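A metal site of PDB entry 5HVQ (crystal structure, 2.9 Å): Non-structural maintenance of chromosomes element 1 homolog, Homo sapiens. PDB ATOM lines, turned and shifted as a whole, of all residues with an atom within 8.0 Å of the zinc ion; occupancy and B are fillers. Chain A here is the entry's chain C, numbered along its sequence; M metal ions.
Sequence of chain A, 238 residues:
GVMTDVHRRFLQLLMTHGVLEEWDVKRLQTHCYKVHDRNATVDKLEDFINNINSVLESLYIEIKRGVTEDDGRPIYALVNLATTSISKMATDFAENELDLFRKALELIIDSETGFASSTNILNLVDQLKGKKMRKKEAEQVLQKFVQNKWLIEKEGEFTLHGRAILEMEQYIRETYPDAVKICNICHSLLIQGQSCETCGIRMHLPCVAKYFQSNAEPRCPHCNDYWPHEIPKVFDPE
Of the 19 residues printed, 4 come within 4 Å of the zinc ion.
N of Cys 196 sits at hydrogen-bond distance from O of Ile 201.
SG of Cys 220 lies close to N of His 222 (3.6 Å).
The backbone NH of Thr 198 lies close to the side-chain sulfur of Cys 196, at 3.4 Å.
The backbone NH (N) of Ile 201 sits close to the side-chain sulfur (SG) of Cys 199.
The side-chain sulfur of Cys 223 sits close to the backbone NH of Asp 225 (3.6 Å).
The backbone NH (N) of Cys 220 sits at hydrogen-bond distance from the backbone carbonyl oxygen (O) of Asp 225 (2.8 Å).
The zinc ion is bound by the side-chain sulfur of Cys 223 (2.3 Å), the side-chain sulfur of Cys 199 (2.3 Å), the side-chain sulfur of Cys 220 (2.4 Å) and the side-chain sulfur of Cys 196 (2.5 Å).
The zinc ion has four donor atoms within binding distance.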
ATOM      1  N   SER A 195      22.761 -11.783  16.808  1.00  0.00           N
ATOM      2  CA  SER A 195      23.648 -10.662  17.081  1.00  0.00           C
ATOM      3  C   SER A 195      24.785 -10.610  16.078  1.00  0.00           C
ATOM      4  O   SER A 195      25.256 -11.639  15.599  1.00  0.00           O
ATOM      5  CB  SER A 195      24.213 -10.764  18.509  1.00  0.00           C
ATOM      6  OG  SER A 195      24.976 -11.945  18.666  1.00  0.00           O
ATOM      7  N   CYS A 196      25.229  -9.392  15.763  1.00  0.00           N
ATOM      8  CA  CYS A 196      26.377  -9.202  14.887  1.00  0.00           C
ATOM      9  C   CYS A 196      27.646  -9.589  15.646  1.00  0.00           C
ATOM     10  O   CYS A 196      27.700  -9.497  16.869  1.00  0.00           O
ATOM     11  CB  CYS A 196      26.462  -7.757  14.400  1.00  0.00           C
ATOM     12  SG  CYS A 196      27.800  -7.437  13.239  1.00  0.00           S
ATOM     13  N   GLU A 197      28.660 -10.030  14.915  1.00  0.00           N
ATOM     14  CA  GLU A 197      29.904 -10.459  15.528  1.00  0.00           C
ATOM     15  C   GLU A 197      31.010  -9.429  15.348  1.00  0.00           C
ATOM     16  O   GLU A 197      32.076  -9.521  15.961  1.00  0.00           O
ATOM     17  CB  GLU A 197      30.343 -11.809  14.953  1.00  0.00           C
ATOM     18  CG  GLU A 197      29.338 -12.932  15.230  1.00  0.00           C
ATOM     19  CD  GLU A 197      29.749 -14.249  14.609  1.00  0.00           C
ATOM     20  OE1 GLU A 197      30.810 -14.307  13.956  1.00  0.00           O
ATOM     21  OE2 GLU A 197      29.001 -15.238  14.775  1.00  0.00           O
ATOM     22  N   THR A 198      30.741  -8.422  14.516  1.00  0.00           N
ATOM     23  CA  THR A 198      31.638  -7.283  14.388  1.00  0.00           C
ATOM     24  C   THR A 198      31.364  -6.304  15.520  1.00  0.00           C
ATOM     25  O   THR A 198      32.228  -6.051  16.365  1.00  0.00           O
ATOM     26  CB  THR A 198      31.470  -6.560  13.036  1.00  0.00           C
ATOM     27  OG1 THR A 198      31.718  -7.487  11.964  1.00  0.00           O
ATOM     28  CG2 THR A 198      32.444  -5.395  12.927  1.00  0.00           C
ATOM     29  N   CYS A 199      30.157  -5.755  15.546  1.00  0.00           N
ATOM     30  CA  CYS A 199      29.697  -4.964  16.671  1.00  0.00           C
ATOM     31  C   CYS A 199      28.882  -5.850  17.610  1.00  0.00           C
ATOM     32  O   CYS A 199      29.094  -7.068  17.638  1.00  0.00           O
ATOM     33  CB  CYS A 199      28.863  -3.757  16.207  1.00  0.00           C
ATOM     34  SG  CYS A 199      27.329  -4.188  15.346  1.00  0.00           S
ATOM     35  N   GLY A 200      27.966  -5.269  18.362  1.00  0.00           N
ATOM     36  CA  GLY A 200      27.213  -6.032  19.345  1.00  0.00           C
ATOM     37  C   GLY A 200      25.709  -5.854  19.306  1.00  0.00           C
ATOM     38  O   GLY A 200      25.023  -6.210  20.267  1.00  0.00           O
ATOM     39  N   ILE A 201      25.192  -5.301  18.221  1.00  0.00           N
ATOM     40  CA  ILE A 201      23.754  -5.079  18.118  1.00  0.00           C
ATOM     41  C   ILE A 201      23.008  -6.393  17.958  1.00  0.00           C
ATOM     42  O   ILE A 201      23.586  -7.390  17.523  1.00  0.00           O
ATOM     43  CB  ILE A 201      23.388  -4.132  16.947  1.00  0.00           C
ATOM     44  CG1 ILE A 201      23.484  -4.868  15.610  1.00  0.00           C
ATOM     45  CG2 ILE A 201      24.287  -2.903  16.958  1.00  0.00           C
ATOM     46  CD1 ILE A 201      22.820  -4.131  14.463  1.00  0.00           C
ATOM     47  N   ARG A 202      21.730  -6.396  18.323  1.00  0.00           N
ATOM     48  CA  ARG A 202      20.911  -7.607  18.241  1.00  0.00           C
ATOM     49  C   ARG A 202      19.600  -7.338  17.511  1.00  0.00           C
ATOM     50  O   ARG A 202      19.109  -6.207  17.505  1.00  0.00           O
ATOM     51  CB  ARG A 202      20.638  -8.160  19.637  1.00  0.00           C
ATOM     52  CG  ARG A 202      21.865  -8.689  20.367  1.00  0.00           C
ATOM     53  CD  ARG A 202      21.477  -9.304  21.698  1.00  0.00           C
ATOM     54  NE  ARG A 202      22.576 -10.049  22.312  1.00  0.00           N
ATOM     55  CZ  ARG A 202      23.443  -9.533  23.182  1.00  0.00           C
ATOM     56  NH1 ARG A 202      23.340  -8.256  23.543  1.00  0.00           N
ATOM     57  NH2 ARG A 202      24.411 -10.286  23.687  1.00  0.00           N
ATOM     58  N   MET A 203      19.039  -8.380  16.909  1.00  0.00           N
ATOM     59  CA  MET A 203      17.772  -8.264  16.188  1.00  0.00           C
ATOM     60  C   MET A 203      16.835  -9.411  16.516  1.00  0.00           C
ATOM     61  O   MET A 203      17.255 -10.553  16.660  1.00  0.00           O
ATOM     62  CB  MET A 203      17.995  -8.223  14.676  1.00  0.00           C
ATOM     63  CG  MET A 203      18.854  -7.081  14.180  1.00  0.00           C
ATOM     64  SD  MET A 203      18.839  -7.037  12.376  1.00  0.00           S
ATOM     65  CE  MET A 203      20.480  -6.412  12.055  1.00  0.00           C
ATOM     66  N   ARG A 219      23.714  -7.071   5.134  1.00  0.00           N
ATOM     67  CA  ARG A 219      24.751  -6.336   5.852  1.00  0.00           C
ATOM     68  C   ARG A 219      24.197  -5.711   7.132  1.00  0.00           C
ATOM     69  O   ARG A 219      23.092  -5.168   7.130  1.00  0.00           O
ATOM     70  CB  ARG A 219      25.369  -5.254   4.970  1.00  0.00           C
ATOM     71  CG  ARG A 219      26.212  -5.782   3.815  1.00  0.00           C
ATOM     72  CD  ARG A 219      26.786  -4.633   2.991  1.00  0.00           C
ATOM     73  NE  ARG A 219      27.661  -5.090   1.922  1.00  0.00           N
ATOM     74  CZ  ARG A 219      28.981  -5.209   2.035  1.00  0.00           C
ATOM     75  NH1 ARG A 219      29.578  -4.909   3.181  1.00  0.00           N
ATOM     76  NH2 ARG A 219      29.699  -5.642   1.007  1.00  0.00           N
ATOM     77  N   CYS A 220      24.971  -5.792   8.209  1.00  0.00           N
ATOM     78  CA  CYS A 220      24.575  -5.195   9.485  1.00  0.00           C
ATOM     79  C   CYS A 220      24.420  -3.685   9.366  1.00  0.00           C
ATOM     80  O   CYS A 220      25.379  -2.969   9.093  1.00  0.00           O
ATOM     81  CB  CYS A 220      25.619  -5.528  10.563  1.00  0.00           C
ATOM     82  SG  CYS A 220      25.429  -4.576  12.087  1.00  0.00           S
ATOM     83  N   PRO A 221      23.194  -3.187   9.587  1.00  0.00           N
ATOM     84  CA  PRO A 221      22.827  -1.770   9.429  1.00  0.00           C
ATOM     85  C   PRO A 221      23.711  -0.792  10.202  1.00  0.00           C
ATOM     86  O   PRO A 221      23.752   0.385   9.855  1.00  0.00           O
ATOM     87  CB  PRO A 221      21.389  -1.716   9.967  1.00  0.00           C
ATOM     88  CG  PRO A 221      21.210  -2.966  10.769  1.00  0.00           C
ATOM     89  CD  PRO A 221      22.063  -3.983  10.090  1.00  0.00           C
ATOM     90  N   HIS A 222      24.409  -1.285  11.220  1.00  0.00           N
ATOM     91  CA  HIS A 222      25.231  -0.404  12.051  1.00  0.00           C
ATOM     92  C   HIS A 222      26.672  -0.327  11.573  1.00  0.00           C
ATOM     93  O   HIS A 222      27.263   0.757  11.537  1.00  0.00           O
ATOM     94  CB  HIS A 222      25.182  -0.867  13.514  1.00  0.00           C
ATOM     95  CG  HIS A 222      25.830   0.096  14.467  1.00  0.00           C
ATOM     96  ND1 HIS A 222      26.932  -0.249  15.220  1.00  0.00           N
ATOM     97  CD2 HIS A 222      25.535   1.375  14.779  1.00  0.00           C
ATOM     98  CE1 HIS A 222      27.283   0.793  15.966  1.00  0.00           C
ATOM     99  NE2 HIS A 222      26.457   1.783  15.720  1.00  0.00           N
ATOM    100  N   CYS A 223      27.253  -1.464  11.200  1.00  0.00           N
ATOM    101  CA  CYS A 223      28.658  -1.514  10.813  1.00  0.00           C
ATOM    102  C   CYS A 223      28.863  -1.933   9.362  1.00  0.00           C
ATOM    103  O   CYS A 223      30.005  -1.994   8.881  1.00  0.00           O
ATOM    104  CB  CYS A 223      29.431  -2.455  11.736  1.00  0.00           C
ATOM    105  SG  CYS A 223      28.983  -4.192  11.570  1.00  0.00           S
ATOM    106  N   ASN A 224      27.766  -2.231   8.668  1.00  0.00           N
ATOM    107  CA  ASN A 224      27.783  -2.605   7.251  1.00  0.00           C
ATOM    108  C   ASN A 224      28.662  -3.824   6.960  1.00  0.00           C
ATOM    109  O   ASN A 224      29.164  -3.979   5.849  1.00  0.00           O
ATOM    110  CB  ASN A 224      28.238  -1.417   6.400  1.00  0.00           C
ATOM    111  CG  ASN A 224      27.794  -1.537   4.956  1.00  0.00           C
ATOM    112  OD1 ASN A 224      28.605  -1.794   4.067  1.00  0.00           O
ATOM    113  ND2 ASN A 224      26.506  -1.349   4.723  1.00  0.00           N
ATOM    114  N   ASP A 225      28.828  -4.686   7.957  1.00  0.00           N
ATOM    115  CA  ASP A 225      29.564  -5.930   7.759  1.00  0.00           C
ATOM    116  C   ASP A 225      28.594  -7.044   7.381  1.00  0.00           C
ATOM    117  O   ASP A 225      27.411  -6.969   7.695  1.00  0.00           O
ATOM    118  CB  ASP A 225      30.350  -6.303   9.013  1.00  0.00           C
ATOM    119  CG  ASP A 225      31.492  -7.266   8.735  1.00  0.00           C
ATOM    120  OD1 ASP A 225      31.342  -8.129   7.831  1.00  0.00           O
ATOM    121  OD2 ASP A 225      32.535  -7.176   9.409  1.00  0.00           O
ATOM    122  N   TYR A 226      29.100  -8.058   6.695  1.00  0.00           N
ATOM    123  CA  TYR A 226      28.271  -9.164   6.222  1.00  0.00           C
ATOM    124  C   TYR A 226      27.592  -9.893   7.379  1.00  0.00           C
ATOM    125  O   TYR A 226      28.239 -10.238   8.365  1.00  0.00           O
ATOM    126  CB  TYR A 226      29.105 -10.145   5.392  1.00  0.00           C
ATOM    127  CG  TYR A 226      29.868  -9.497   4.264  1.00  0.00           C
ATOM    128  CD1 TYR A 226      31.190  -9.077   4.432  1.00  0.00           C
ATOM    129  CD2 TYR A 226      29.283  -9.304   3.014  1.00  0.00           C
ATOM    130  CE1 TYR A 226      31.881  -8.484   3.395  1.00  0.00           C
ATOM    131  CE2 TYR A 226      29.978  -8.718   1.983  1.00  0.00           C
ATOM    132  CZ  TYR A 226      31.279  -8.301   2.181  1.00  0.00           C
ATOM    133  OH  TYR A 226      31.974  -7.716   1.149  1.00  0.00           O
ATOM    134  N   TRP A 227      26.290 -10.126   7.246  1.00  0.00           N
ATOM    135  CA  TRP A 227      25.517 -10.780   8.293  1.00  0.00           C
ATOM    136  C   TRP A 227      25.840 -12.269   8.374  1.00  0.00           C
ATOM    137  O   TRP A 227      25.608 -13.011   7.421  1.00  0.00           O
ATOM    138  CB  TRP A 227      24.018 -10.572   8.056  1.00  0.00           C
ATOM    139  CG  TRP A 227      23.187 -10.878   9.266  1.00  0.00           C
ATOM    140  CD1 TRP A 227      22.343 -11.945   9.426  1.00  0.00           C
ATOM    141  CD2 TRP A 227      23.128 -10.128  10.478  1.00  0.00           C
ATOM    142  NE1 TRP A 227      21.757 -11.888  10.671  1.00  0.00           N
ATOM    143  CE2 TRP A 227      22.224 -10.789  11.335  1.00  0.00           C
ATOM    144  CE3 TRP A 227      23.749  -8.962  10.926  1.00  0.00           C
ATOM    145  CZ2 TRP A 227      21.935 -10.318  12.611  1.00  0.00           C
ATOM    146  CZ3 TRP A 227      23.463  -8.496  12.193  1.00  0.00           C
ATOM    147  CH2 TRP A 227      22.552  -9.167  13.020  1.00  0.00           C
ATOM    148  N   PRO A 228      26.379 -12.707   9.520  1.00  0.00           N
ATOM    149  CA  PRO A 228      26.905 -14.062   9.732  1.00  0.00           C
ATOM    150  C   PRO A 228      25.831 -15.137   9.816  1.00  0.00           C
ATOM    151  O   PRO A 228      26.096 -16.289   9.465  1.00  0.00           O
ATOM    152  CB  PRO A 228      27.644 -13.954  11.070  1.00  0.00           C
ATOM    153  CG  PRO A 228      27.779 -12.484  11.345  1.00  0.00           C
ATOM    154  CD  PRO A 228      26.590 -11.850  10.708  1.00  0.00           C
HETATM  155 ZN    ZN M   1      27.492  -4.985  13.158  1.00  0.00          ZN
